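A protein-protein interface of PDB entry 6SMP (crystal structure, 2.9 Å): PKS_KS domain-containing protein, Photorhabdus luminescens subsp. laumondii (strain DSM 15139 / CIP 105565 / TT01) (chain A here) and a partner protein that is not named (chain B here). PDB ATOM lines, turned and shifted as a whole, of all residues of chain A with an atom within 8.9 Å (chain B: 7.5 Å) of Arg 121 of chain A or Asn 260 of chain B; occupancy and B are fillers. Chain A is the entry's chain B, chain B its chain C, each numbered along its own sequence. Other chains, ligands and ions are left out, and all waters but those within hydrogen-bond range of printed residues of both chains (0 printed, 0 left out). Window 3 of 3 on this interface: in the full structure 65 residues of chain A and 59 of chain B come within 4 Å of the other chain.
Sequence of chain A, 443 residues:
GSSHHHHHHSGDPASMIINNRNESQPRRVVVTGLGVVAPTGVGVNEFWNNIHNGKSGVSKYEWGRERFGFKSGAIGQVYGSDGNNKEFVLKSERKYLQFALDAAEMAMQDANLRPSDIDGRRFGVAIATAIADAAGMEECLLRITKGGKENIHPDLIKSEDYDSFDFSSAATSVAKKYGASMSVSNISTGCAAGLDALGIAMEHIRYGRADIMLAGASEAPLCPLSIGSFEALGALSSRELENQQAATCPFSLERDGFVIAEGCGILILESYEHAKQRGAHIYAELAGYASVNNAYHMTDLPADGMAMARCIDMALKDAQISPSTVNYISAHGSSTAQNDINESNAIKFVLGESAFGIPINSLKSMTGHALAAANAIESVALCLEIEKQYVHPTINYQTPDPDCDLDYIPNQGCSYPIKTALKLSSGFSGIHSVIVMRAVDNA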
ATOM      1  N   ASP A 117      20.082  37.611   0.961  1.00  0.00           N
ATOM      2  CA  ASP A 117      21.237  37.206   0.176  1.00  0.00           C
ATOM      3  C   ASP A 117      21.513  35.716   0.370  1.00  0.00           C
ATOM      4  O   ASP A 117      21.890  35.030  -0.579  1.00  0.00           O
ATOM      5  CB  ASP A 117      22.462  38.062   0.507  1.00  0.00           C
ATOM      6  CG  ASP A 117      22.257  39.556   0.301  1.00  0.00           C
ATOM      7  OD1 ASP A 117      21.503  39.927  -0.623  1.00  0.00           O
ATOM      8  OD2 ASP A 117      22.855  40.338   1.068  1.00  0.00           O
ATOM      9  N   ILE A 118      21.321  35.224   1.601  1.00  0.00           N
ATOM     10  CA  ILE A 118      21.651  33.850   1.955  1.00  0.00           C
ATOM     11  C   ILE A 118      20.496  32.931   1.563  1.00  0.00           C
ATOM     12  O   ILE A 118      19.438  32.957   2.189  1.00  0.00           O
ATOM     13  CB  ILE A 118      21.995  33.717   3.455  1.00  0.00           C
ATOM     14  CG1 ILE A 118      23.133  34.653   3.874  1.00  0.00           C
ATOM     15  CG2 ILE A 118      22.302  32.267   3.813  1.00  0.00           C
ATOM     16  CD1 ILE A 118      23.211  34.901   5.365  1.00  0.00           C
ATOM     17  N   ASP A 119      20.719  32.122   0.520  1.00  0.00           N
ATOM     18  CA  ASP A 119      19.843  31.012   0.182  1.00  0.00           C
ATOM     19  C   ASP A 119      20.389  29.756   0.858  1.00  0.00           C
ATOM     20  O   ASP A 119      21.494  29.316   0.547  1.00  0.00           O
ATOM     21  CB  ASP A 119      19.720  30.835  -1.335  1.00  0.00           C
ATOM     22  CG  ASP A 119      18.709  29.783  -1.768  1.00  0.00           C
ATOM     23  OD1 ASP A 119      18.709  29.435  -2.965  1.00  0.00           O
ATOM     24  OD2 ASP A 119      17.920  29.329  -0.913  1.00  0.00           O
ATOM     25  N   GLY A 120      19.597  29.192   1.781  1.00  0.00           N
ATOM     26  CA  GLY A 120      20.010  28.089   2.634  1.00  0.00           C
ATOM     27  C   GLY A 120      20.554  26.893   1.855  1.00  0.00           C
ATOM     28  O   GLY A 120      21.544  26.289   2.262  1.00  0.00           O
ATOM     29  N   ARG A 121      19.905  26.575   0.728  1.00  0.00           N
ATOM     30  CA  ARG A 121      20.235  25.406  -0.074  1.00  0.00           C
ATOM     31  C   ARG A 121      21.500  25.648  -0.895  1.00  0.00           C
ATOM     32  O   ARG A 121      22.069  24.703  -1.441  1.00  0.00           O
ATOM     33  CB  ARG A 121      19.072  25.050  -1.005  1.00  0.00           C
ATOM     34  CG  ARG A 121      17.815  24.577  -0.290  1.00  0.00           C
ATOM     35  CD  ARG A 121      16.697  24.325  -1.283  1.00  0.00           C
ATOM     36  NE  ARG A 121      15.424  24.015  -0.647  1.00  0.00           N
ATOM     37  CZ  ARG A 121      14.595  24.917  -0.130  1.00  0.00           C
ATOM     38  NH1 ARG A 121      14.906  26.202  -0.155  1.00  0.00           N
ATOM     39  NH2 ARG A 121      13.459  24.527   0.422  1.00  0.00           N
ATOM     40  N   ARG A 122      21.931  26.914  -0.980  1.00  0.00           N
ATOM     41  CA  ARG A 122      23.090  27.299  -1.774  1.00  0.00           C
ATOM     42  C   ARG A 122      24.253  27.711  -0.871  1.00  0.00           C
ATOM     43  O   ARG A 122      25.304  28.116  -1.364  1.00  0.00           O
ATOM     44  CB  ARG A 122      22.733  28.445  -2.728  1.00  0.00           C
ATOM     45  CG  ARG A 122      21.575  28.152  -3.673  1.00  0.00           C
ATOM     46  CD  ARG A 122      21.956  27.301  -4.870  1.00  0.00           C
ATOM     47  NE  ARG A 122      22.816  28.015  -5.806  1.00  0.00           N
ATOM     48  CZ  ARG A 122      23.407  27.468  -6.864  1.00  0.00           C
ATOM     49  NH1 ARG A 122      23.239  26.185  -7.137  1.00  0.00           N
ATOM     50  NH2 ARG A 122      24.168  28.211  -7.648  1.00  0.00           N
ATOM     51  N   PHE A 123      24.059  27.610   0.450  1.00  0.00           N
ATOM     52  CA  PHE A 123      25.060  28.017   1.426  1.00  0.00           C
ATOM     53  C   PHE A 123      25.606  26.782   2.141  1.00  0.00           C
ATOM     54  O   PHE A 123      24.857  26.074   2.810  1.00  0.00           O
ATOM     55  CB  PHE A 123      24.465  29.048   2.392  1.00  0.00           C
ATOM     56  CG  PHE A 123      25.344  29.455   3.551  1.00  0.00           C
ATOM     57  CD1 PHE A 123      24.826  29.560   4.834  1.00  0.00           C
ATOM     58  CD2 PHE A 123      26.688  29.744   3.362  1.00  0.00           C
ATOM     59  CE1 PHE A 123      25.631  29.935   5.899  1.00  0.00           C
ATOM     60  CE2 PHE A 123      27.494  30.120   4.428  1.00  0.00           C
ATOM     61  CZ  PHE A 123      26.964  30.216   5.695  1.00  0.00           C
ATOM     62  N   GLY A 124      26.911  26.528   1.983  1.00  0.00           N
ATOM     63  CA  GLY A 124      27.552  25.355   2.561  1.00  0.00           C
ATOM     64  C   GLY A 124      28.709  25.713   3.492  1.00  0.00           C
ATOM     65  O   GLY A 124      29.116  26.872   3.561  1.00  0.00           O
ATOM     66  N   TYR A 178      23.947  29.457  11.188  1.00  0.00           N
ATOM     67  CA  TYR A 178      23.738  30.395  10.092  1.00  0.00           C
ATOM     68  C   TYR A 178      22.815  29.818   9.017  1.00  0.00           C
ATOM     69  O   TYR A 178      22.507  30.501   8.041  1.00  0.00           O
ATOM     70  CB  TYR A 178      25.076  30.878   9.524  1.00  0.00           C
ATOM     71  CG  TYR A 178      25.967  31.528  10.550  1.00  0.00           C
ATOM     72  CD1 TYR A 178      27.142  30.922  10.964  1.00  0.00           C
ATOM     73  CD2 TYR A 178      25.615  32.733  11.139  1.00  0.00           C
ATOM     74  CE1 TYR A 178      27.956  31.505  11.922  1.00  0.00           C
ATOM     75  CE2 TYR A 178      26.415  33.330  12.099  1.00  0.00           C
ATOM     76  CZ  TYR A 178      27.590  32.714  12.491  1.00  0.00           C
ATOM     77  OH  TYR A 178      28.385  33.297  13.434  1.00  0.00           O
ATOM     78  N   GLY A 179      22.377  28.567   9.205  1.00  0.00           N
ATOM     79  CA  GLY A 179      21.371  27.952   8.353  1.00  0.00           C
ATOM     80  C   GLY A 179      21.927  27.501   7.005  1.00  0.00           C
ATOM     81  O   GLY A 179      21.352  27.810   5.961  1.00  0.00           O
ATOM     82  N   ALA A 180      23.036  26.754   7.047  1.00  0.00           N
ATOM     83  CA  ALA A 180      23.684  26.237   5.852  1.00  0.00           C
ATOM     84  C   ALA A 180      23.152  24.841   5.534  1.00  0.00           C
ATOM     85  O   ALA A 180      23.542  23.866   6.174  1.00  0.00           O
ATOM     86  CB  ALA A 180      25.180  26.233   6.047  1.00  0.00           C
ATOM     87  N   SER A 181      22.264  24.759   4.534  1.00  0.00           N
ATOM     88  CA  SER A 181      21.611  23.511   4.165  1.00  0.00           C
ATOM     89  C   SER A 181      22.325  22.726   3.063  1.00  0.00           C
ATOM     90  O   SER A 181      21.941  21.597   2.760  1.00  0.00           O
ATOM     91  CB  SER A 181      20.176  23.798   3.731  1.00  0.00           C
ATOM     92  OG  SER A 181      19.494  24.535   4.752  1.00  0.00           O
ATOM     93  N   MET A 182      23.360  23.334   2.469  1.00  0.00           N
ATOM     94  CA  MET A 182      24.170  22.711   1.434  1.00  0.00           C
ATOM     95  C   MET A 182      25.340  21.976   2.095  1.00  0.00           C
ATOM     96  O   MET A 182      25.554  22.124   3.296  1.00  0.00           O
ATOM     97  CB  MET A 182      24.649  23.784   0.445  1.00  0.00           C
ATOM     98  CG  MET A 182      26.002  23.539  -0.198  1.00  0.00           C
ATOM     99  SD  MET A 182      25.971  22.321  -1.533  1.00  0.00           S
ATOM    100  CE  MET A 182      27.480  22.761  -2.390  1.00  0.00           C
ATOM    101  N   SER A 183      26.069  21.164   1.314  1.00  0.00           N
ATOM    102  CA  SER A 183      27.199  20.371   1.781  1.00  0.00           C
ATOM    103  C   SER A 183      27.956  20.923   2.990  1.00  0.00           C
ATOM    104  O   SER A 183      28.558  21.995   2.919  1.00  0.00           O
ATOM    105  CB  SER A 183      28.181  20.195   0.620  1.00  0.00           C
ATOM    106  OG  SER A 183      29.339  19.463   1.045  1.00  0.00           O
ATOM    107  N   GLY A 208      28.523  25.603  -9.953  1.00  0.00           N
ATOM    108  CA  GLY A 208      27.100  25.911  -9.895  1.00  0.00           C
ATOM    109  C   GLY A 208      26.329  25.157  -8.810  1.00  0.00           C
ATOM    110  O   GLY A 208      25.133  24.917  -8.966  1.00  0.00           O
ATOM    111  N   ARG A 209      27.011  24.803  -7.713  1.00  0.00           N
ATOM    112  CA  ARG A 209      26.388  24.079  -6.614  1.00  0.00           C
ATOM    113  C   ARG A 209      26.041  25.036  -5.474  1.00  0.00           C
ATOM    114  O   ARG A 209      25.018  24.862  -4.813  1.00  0.00           O
ATOM    115  CB  ARG A 209      27.294  22.946  -6.119  1.00  0.00           C
ATOM    116  CG  ARG A 209      26.985  21.584  -6.724  1.00  0.00           C
ATOM    117  CD  ARG A 209      28.089  20.586  -6.426  1.00  0.00           C
ATOM    118  NE  ARG A 209      29.118  20.592  -7.457  1.00  0.00           N
ATOM    119  CZ  ARG A 209      30.374  20.187  -7.289  1.00  0.00           C
ATOM    120  NH1 ARG A 209      30.784  19.746  -6.111  1.00  0.00           N
ATOM    121  NH2 ARG A 209      31.219  20.236  -8.302  1.00  0.00           N
ATOM    122  N   ALA A 210      26.904  26.035  -5.249  1.00  0.00           N
ATOM    123  CA  ALA A 210      26.745  26.962  -4.140  1.00  0.00           C
ATOM    124  C   ALA A 210      26.958  28.398  -4.614  1.00  0.00           C
ATOM    125  O   ALA A 210      27.657  28.639  -5.597  1.00  0.00           O
ATOM    126  CB  ALA A 210      27.703  26.600  -3.031  1.00  0.00           C
ATOM    127  N   ASP A 211      26.337  29.342  -3.892  1.00  0.00           N
ATOM    128  CA  ASP A 211      26.534  30.767  -4.104  1.00  0.00           C
ATOM    129  C   ASP A 211      27.463  31.312  -3.024  1.00  0.00           C
ATOM    130  O   ASP A 211      28.394  32.051  -3.330  1.00  0.00           O
ATOM    131  CB  ASP A 211      25.203  31.524  -4.132  1.00  0.00           C
ATOM    132  CG  ASP A 211      24.305  31.146  -5.298  1.00  0.00           C
ATOM    133  OD1 ASP A 211      24.835  30.952  -6.412  1.00  0.00           O
ATOM    134  OD2 ASP A 211      23.081  31.049  -5.083  1.00  0.00           O
ATOM    135  N   ILE A 212      27.188  30.943  -1.764  1.00  0.00           N
ATOM    136  CA  ILE A 212      28.018  31.294  -0.620  1.00  0.00           C
ATOM    137  C   ILE A 212      28.634  30.011  -0.062  1.00  0.00           C
ATOM    138  O   ILE A 212      28.051  28.936  -0.191  1.00  0.00           O
ATOM    139  CB  ILE A 212      27.201  32.045   0.455  1.00  0.00           C
ATOM    140  CG1 ILE A 212      26.344  33.164  -0.145  1.00  0.00           C
ATOM    141  CG2 ILE A 212      28.109  32.570   1.561  1.00  0.00           C
ATOM    142  CD1 ILE A 212      25.236  33.652   0.760  1.00  0.00           C
ATOM    143  N   MET A 213      29.810  30.139   0.568  1.00  0.00           N
ATOM    144  CA  MET A 213      30.510  29.001   1.148  1.00  0.00           C
ATOM    145  C   MET A 213      31.416  29.469   2.287  1.00  0.00           C
ATOM    146  O   MET A 213      32.311  30.286   2.077  1.00  0.00           O
ATOM    147  CB  MET A 213      31.352  28.289   0.084  1.00  0.00           C
ATOM    148  CG  MET A 213      31.575  26.819   0.369  1.00  0.00           C
ATOM    149  SD  MET A 213      30.114  25.806   0.032  1.00  0.00           S
ATOM    150  CE  MET A 213      30.630  24.250   0.756  1.00  0.00           C
ATOM    151  N   ASP B 249      24.707  15.585  -1.320  1.00  0.00           N
ATOM    152  CA  ASP B 249      25.346  16.053  -0.099  1.00  0.00           C
ATOM    153  C   ASP B 249      24.631  17.308   0.398  1.00  0.00           C
ATOM    154  O   ASP B 249      24.862  18.402  -0.113  1.00  0.00           O
ATOM    155  CB  ASP B 249      26.850  16.274  -0.299  1.00  0.00           C
ATOM    156  CG  ASP B 249      27.627  16.534   0.983  1.00  0.00           C
ATOM    157  OD1 ASP B 249      28.843  16.793   0.884  1.00  0.00           O
ATOM    158  OD2 ASP B 249      27.018  16.472   2.072  1.00  0.00           O
ATOM    159  N   TYR B 250      23.764  17.128   1.403  1.00  0.00           N
ATOM    160  CA  TYR B 250      22.995  18.221   1.978  1.00  0.00           C
ATOM    161  C   TYR B 250      23.033  18.153   3.503  1.00  0.00           C
ATOM    162  O   TYR B 250      23.544  17.193   4.078  1.00  0.00           O
ATOM    163  CB  TYR B 250      21.555  18.200   1.458  1.00  0.00           C
ATOM    164  CG  TYR B 250      21.386  18.672   0.037  1.00  0.00           C
ATOM    165  CD1 TYR B 250      20.862  17.836  -0.937  1.00  0.00           C
ATOM    166  CD2 TYR B 250      21.753  19.956  -0.339  1.00  0.00           C
ATOM    167  CE1 TYR B 250      20.706  18.261  -2.247  1.00  0.00           C
ATOM    168  CE2 TYR B 250      21.604  20.397  -1.644  1.00  0.00           C
ATOM    169  CZ  TYR B 250      21.079  19.547  -2.602  1.00  0.00           C
ATOM    170  OH  TYR B 250      20.928  19.975  -3.889  1.00  0.00           O
ATOM    171  N   PHE B 251      22.478  19.194   4.136  1.00  0.00           N
ATOM    172  CA  PHE B 251      22.438  19.319   5.583  1.00  0.00           C
ATOM    173  C   PHE B 251      21.069  19.846   6.006  1.00  0.00           C
ATOM    174  O   PHE B 251      20.441  20.612   5.277  1.00  0.00           O
ATOM    175  CB  PHE B 251      23.555  20.249   6.060  1.00  0.00           C
ATOM    176  CG  PHE B 251      23.774  20.275   7.552  1.00  0.00           C
ATOM    177  CD1 PHE B 251      24.497  19.273   8.182  1.00  0.00           C
ATOM    178  CD2 PHE B 251      23.268  21.309   8.326  1.00  0.00           C
ATOM    179  CE1 PHE B 251      24.700  19.297   9.553  1.00  0.00           C
ATOM    180  CE2 PHE B 251      23.473  21.335   9.698  1.00  0.00           C
ATOM    181  CZ  PHE B 251      24.189  20.329  10.309  1.00  0.00           C
ATOM    182  N   LYS B 255      14.015  20.626  11.540  1.00  0.00           N
ATOM    183  CA  LYS B 255      13.048  19.650  11.054  1.00  0.00           C
ATOM    184  C   LYS B 255      12.273  20.175   9.844  1.00  0.00           C
ATOM    185  O   LYS B 255      11.705  19.384   9.093  1.00  0.00           O
ATOM    186  CB  LYS B 255      12.082  19.233  12.168  1.00  0.00           C
ATOM    187  CG  LYS B 255      12.671  18.320  13.234  1.00  0.00           C
ATOM    188  CD  LYS B 255      11.621  17.651  14.093  1.00  0.00           C
ATOM    189  CE  LYS B 255      12.206  16.639  15.055  1.00  0.00           C
ATOM    190  NZ  LYS B 255      11.148  15.886  15.769  1.00  0.00           N
ATOM    191  N   ASN B 256      12.243  21.503   9.666  1.00  0.00           N
ATOM    192  CA  ASN B 256      11.552  22.116   8.541  1.00  0.00           C
ATOM    193  C   ASN B 256      12.274  21.776   7.239  1.00  0.00           C
ATOM    194  O   ASN B 256      11.640  21.403   6.253  1.00  0.00           O
ATOM    195  CB  ASN B 256      11.408  23.633   8.704  1.00  0.00           C
ATOM    196  CG  ASN B 256      10.473  24.033   9.826  1.00  0.00           C
ATOM    197  OD1 ASN B 256      10.856  24.793  10.713  1.00  0.00           O
ATOM    198  ND2 ASN B 256       9.250  23.532   9.799  1.00  0.00           N
ATOM    199  N   THR B 257      13.607  21.907   7.259  1.00  0.00           N
ATOM    200  CA  THR B 257      14.445  21.663   6.094  1.00  0.00           C
ATOM    201  C   THR B 257      14.565  20.164   5.819  1.00  0.00           C
ATOM    202  O   THR B 257      14.811  19.770   4.681  1.00  0.00           O
ATOM    203  CB  THR B 257      15.830  22.304   6.249  1.00  0.00           C
ATOM    204  OG1 THR B 257      16.394  21.867   7.485  1.00  0.00           O
ATOM    205  CG2 THR B 257      15.796  23.817   6.203  1.00  0.00           C
ATOM    206  N   ARG B 258      14.380  19.343   6.864  1.00  0.00           N
ATOM    207  CA  ARG B 258      14.581  17.901   6.809  1.00  0.00           C
ATOM    208  C   ARG B 258      13.748  17.280   5.687  1.00  0.00           C
ATOM    209  O   ARG B 258      14.253  16.459   4.925  1.00  0.00           O
ATOM    210  CB  ARG B 258      14.243  17.272   8.167  1.00  0.00           C
ATOM    211  CG  ARG B 258      14.474  15.769   8.254  1.00  0.00           C
ATOM    212  CD  ARG B 258      13.951  15.177   9.551  1.00  0.00           C
ATOM    213  NE  ARG B 258      12.500  15.253   9.665  1.00  0.00           N
ATOM    214  CZ  ARG B 258      11.786  14.826  10.704  1.00  0.00           C
ATOM    215  NH1 ARG B 258      10.469  14.947  10.692  1.00  0.00           N
ATOM    216  NH2 ARG B 258      12.383  14.279  11.748  1.00  0.00           N
ATOM    217  N   ASN B 259      12.474  17.685   5.599  1.00  0.00           N
ATOM    218  CA  ASN B 259      11.529  17.127   4.644  1.00  0.00           C
ATOM    219  C   ASN B 259      11.878  17.581   3.227  1.00  0.00           C
ATOM    220  O   ASN B 259      11.777  16.796   2.285  1.00  0.00           O
ATOM    221  CB  ASN B 259      10.083  17.471   5.008  1.00  0.00           C
ATOM    222  CG  ASN B 259       9.618  16.830   6.300  1.00  0.00           C
ATOM    223  OD1 ASN B 259      10.411  16.606   7.213  1.00  0.00           O
ATOM    224  ND2 ASN B 259       8.332  16.537   6.388  1.00  0.00           N
ATOM    225  N   ASN B 260      12.287  18.849   3.094  1.00  0.00           N
ATOM    226  CA  ASN B 260      12.641  19.434   1.810  1.00  0.00           C
ATOM    227  C   ASN B 260      13.956  18.840   1.306  1.00  0.00           C
ATOM    228  O   ASN B 260      14.149  18.709   0.098  1.00  0.00           O
ATOM    229  CB  ASN B 260      12.698  20.964   1.873  1.00  0.00           C
ATOM    230  CG  ASN B 260      11.348  21.612   2.103  1.00  0.00           C
ATOM    231  OD1 ASN B 260      10.336  20.931   2.258  1.00  0.00           O
ATOM    232  ND2 ASN B 260      11.320  22.935   2.126  1.00  0.00           N
ATOM    233  N   THR B 261      14.848  18.484   2.240  1.00  0.00           N
ATOM    234  CA  THR B 261      16.141  17.901   1.911  1.00  0.00           C
ATOM    235  C   THR B 261      15.962  16.489   1.356  1.00  0.00           C
ATOM    236  O   THR B 261      16.664  16.100   0.423  1.00  0.00           O
ATOM    237  CB  THR B 261      17.092  17.906   3.115  1.00  0.00           C
ATOM    238  OG1 THR B 261      17.125  19.222   3.667  1.00  0.00           O
ATOM    239  CG2 THR B 261      18.497  17.488   2.749  1.00  0.00           C
ATOM    240  N   LEU B 262      15.020  15.730   1.934  1.00  0.00           N
ATOM    241  CA  LEU B 262      14.760  14.357   1.527  1.00  0.00           C
ATOM    242  C   LEU B 262      14.151  14.313   0.124  1.00  0.00           C
ATOM    243  O   LEU B 262      14.254  13.294  -0.558  1.00  0.00           O
ATOM    244  CB  LEU B 262      13.841  13.680   2.551  1.00  0.00           C
ATOM    245  CG  LEU B 262      14.483  13.292   3.885  1.00  0.00           C
ATOM    246  CD1 LEU B 262      13.419  13.024   4.938  1.00  0.00           C
ATOM    247  CD2 LEU B 262      15.393  12.083   3.730  1.00  0.00           C
ATOM    248  N   GLU B 263      13.525  15.420  -0.301  1.00  0.00           N
ATOM    249  CA  GLU B 263      12.897  15.514  -1.611  1.00  0.00           C
ATOM    250  C   GLU B 263      13.948  15.688  -2.710  1.00  0.00           C
ATOM    251  O   GLU B 263      13.645  15.484  -3.885  1.00  0.00           O
ATOM    252  CB  GLU B 263      11.872  16.651  -1.653  1.00  0.00           C
ATOM    253  CG  GLU B 263      10.551  16.313  -0.983  1.00  0.00           C
ATOM    254  CD  GLU B 263       9.509  17.421  -1.008  1.00  0.00           C
ATOM    255  OE1 GLU B 263       9.721  18.423  -1.723  1.00  0.00           O
ATOM    256  OE2 GLU B 263       8.485  17.280  -0.310  1.00  0.00           O
ATOM    257  N   TYR B 264      15.174  16.073  -2.329  1.00  0.00           N
ATOM    258  CA  TYR B 264      16.272  16.164  -3.281  1.00  0.00           C
ATOM    259  C   TYR B 264      16.880  14.784  -3.514  1.00  0.00           C
ATOM    260  O   TYR B 264      17.396  14.510  -4.596  1.00  0.00           O
ATOM    261  CB  TYR B 264      17.317  17.194  -2.843  1.00  0.00           C
ATOM    262  CG  TYR B 264      16.917  18.625  -3.096  1.00  0.00           C
ATOM    263  CD1 TYR B 264      16.536  19.455  -2.052  1.00  0.00           C
ATOM    264  CD2 TYR B 264      16.902  19.149  -4.380  1.00  0.00           C
ATOM    265  CE1 TYR B 264      16.159  20.769  -2.275  1.00  0.00           C
ATOM    266  CE2 TYR B 264      16.526  20.461  -4.621  1.00  0.00           C
ATOM    267  CZ  TYR B 264      16.154  21.274  -3.563  1.00  0.00           C
ATOM    268  OH  TYR B 264      15.784  22.566  -3.799  1.00  0.00           O
ATOM    269  N   THR B 265      16.810  13.925  -2.488  1.00  0.00           N
ATOM    270  CA  THR B 265      17.221  12.534  -2.608  1.00  0.00           C
ATOM    271  C   THR B 265      16.260  11.807  -3.544  1.00  0.00           C
ATOM    272  O   THR B 265      16.643  10.844  -4.207  1.00  0.00           O
ATOM    273  CB  THR B 265      17.283  11.840  -1.240  1.00  0.00           C
ATOM    274  OG1 THR B 265      17.968  12.691  -0.320  1.00  0.00           O
ATOM    275  CG2 THR B 265      17.959  10.487  -1.291  1.00  0.00           C
ATOM    276  N   ALA B 266      15.010  12.285  -3.584  1.00  0.00           N
ATOM    277  CA  ALA B 266      13.972  11.728  -4.434  1.00  0.00           C
ATOM    278  C   ALA B 266      14.292  11.983  -5.907  1.00  0.00           C
ATOM    279  O   ALA B 266      14.023  11.131  -6.752  1.00  0.00           O
ATOM    280  CB  ALA B 266      12.634  12.308  -4.046  1.00  0.00           C
ATOM    281  N   ALA B 293       8.185  12.020   2.043  1.00  0.00           N
ATOM    282  CA  ALA B 293       8.900  12.879   1.112  1.00  0.00           C
ATOM    283  C   ALA B 293       8.888  12.266  -0.286  1.00  0.00           C
ATOM    284  O   ALA B 293       8.762  12.985  -1.276  1.00  0.00           O
ATOM    285  CB  ALA B 293      10.307  13.114   1.605  1.00  0.00           C
ATOM    286  N   ASN B 296       5.538  12.529  -2.179  1.00  0.00           N
ATOM    287  CA  ASN B 296       5.317  13.847  -2.755  1.00  0.00           C
ATOM    288  C   ASN B 296       5.905  13.920  -4.165  1.00  0.00           C
ATOM    289  O   ASN B 296       5.426  14.691  -4.994  1.00  0.00           O
ATOM    290  CB  ASN B 296       5.871  14.963  -1.863  1.00  0.00           C
ATOM    291  CG  ASN B 296       5.174  15.073  -0.523  1.00  0.00           C
ATOM    292  OD1 ASN B 296       3.954  14.946  -0.434  1.00  0.00           O
ATOM    293  ND2 ASN B 296       5.940  15.317   0.528  1.00  0.00           N
ATOM    294  N   LYS B 297       6.938  13.105  -4.425  1.00  0.00           N
ATOM    295  CA  LYS B 297       7.659  13.119  -5.692  1.00  0.00           C
ATOM    296  C   LYS B 297       7.280  11.926  -6.575  1.00  0.00           C
ATOM    297  O   LYS B 297       8.012  11.607  -7.512  1.00  0.00           O
ATOM    298  CB  LYS B 297       9.173  13.162  -5.451  1.00  0.00           C
ATOM    299  CG  LYS B 297       9.722  14.475  -4.909  1.00  0.00           C
ATOM    300  CD  LYS B 297       9.813  15.579  -5.944  1.00  0.00           C
ATOM    301  CE  LYS B 297      10.442  16.844  -5.401  1.00  0.00           C
ATOM    302  NZ  LYS B 297      10.575  17.884  -6.447  1.00  0.00           N
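The guanidinium group (NH2) of Arg 121 of chain A lies close to the side-chain amide nitrogen (ND2) of Asn 260 of chain B.
OH of Tyr 264 of chain B sits close to NE of Arg 121 of chain A (3.5 Å).
O of Ser 181 of chain A is in hydrogen-bond range of N of Phe 251 of chain B (2.8 Å).
OD1 of Asp 249 of chain B lies within hydrogen-bond range of OG of Ser 183 of chain A (2.7 Å).
The backbone carbonyl oxygen (O) of Gly 120 of chain A is in hydrogen-bond range of the backbone NH (N) of Ser 181 of chain A (2.8 Å).
The backbone carbonyl oxygen (O) of Gly 120 of chain A lies within hydrogen-bond range of the backbone NH (N) of Met 182 of chain A (3.5 Å).
N of Ser 181 of chain A lies within hydrogen-bond range of O of Phe 123 of chain A (3.4 Å).
O of Phe 123 of chain A is in hydrogen-bond range of N of Met 182 of chain A, 3.1 Å away.
Ala 180 of chain A touches Phe 251 of chain B.
O of Ser 181 of chain A touches CD2 of Tyr 250 of chain B, 3.5 Å away.
O of Met 182 of chain A touches CB of Phe 251 of chain B, 3.9 Å away.
Arg 121 of chain A touches just these residues of chain B: Asn 260 (3.2 Å) and Tyr 264 (3.2 Å).
Of the printed residues of chain B, Met 182 of chain A touches Phe 251 (3.9 Å).
Printed residues of chain A within 4 Å of Tyr 250 of chain B: Ser 181.
Asn 260 of chain B touches one residue of chain A.
Printed residues of chain B that touch a printed residue of chain A: Asp 249, Tyr 250, Phe 251, Asn 260 and Tyr 264.
Hydrophobic or aromatic side chains of chain B that line the printed part of chain A: Tyr 250, Phe 251 and Tyr 264.
Of the 20 printed residues of chain A, 5 touch a printed residue of chain B.
Printed residues of chain A that touch a printed residue of chain B: Arg 121, Ala 180, Ser 181, Met 182 and Ser 183.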
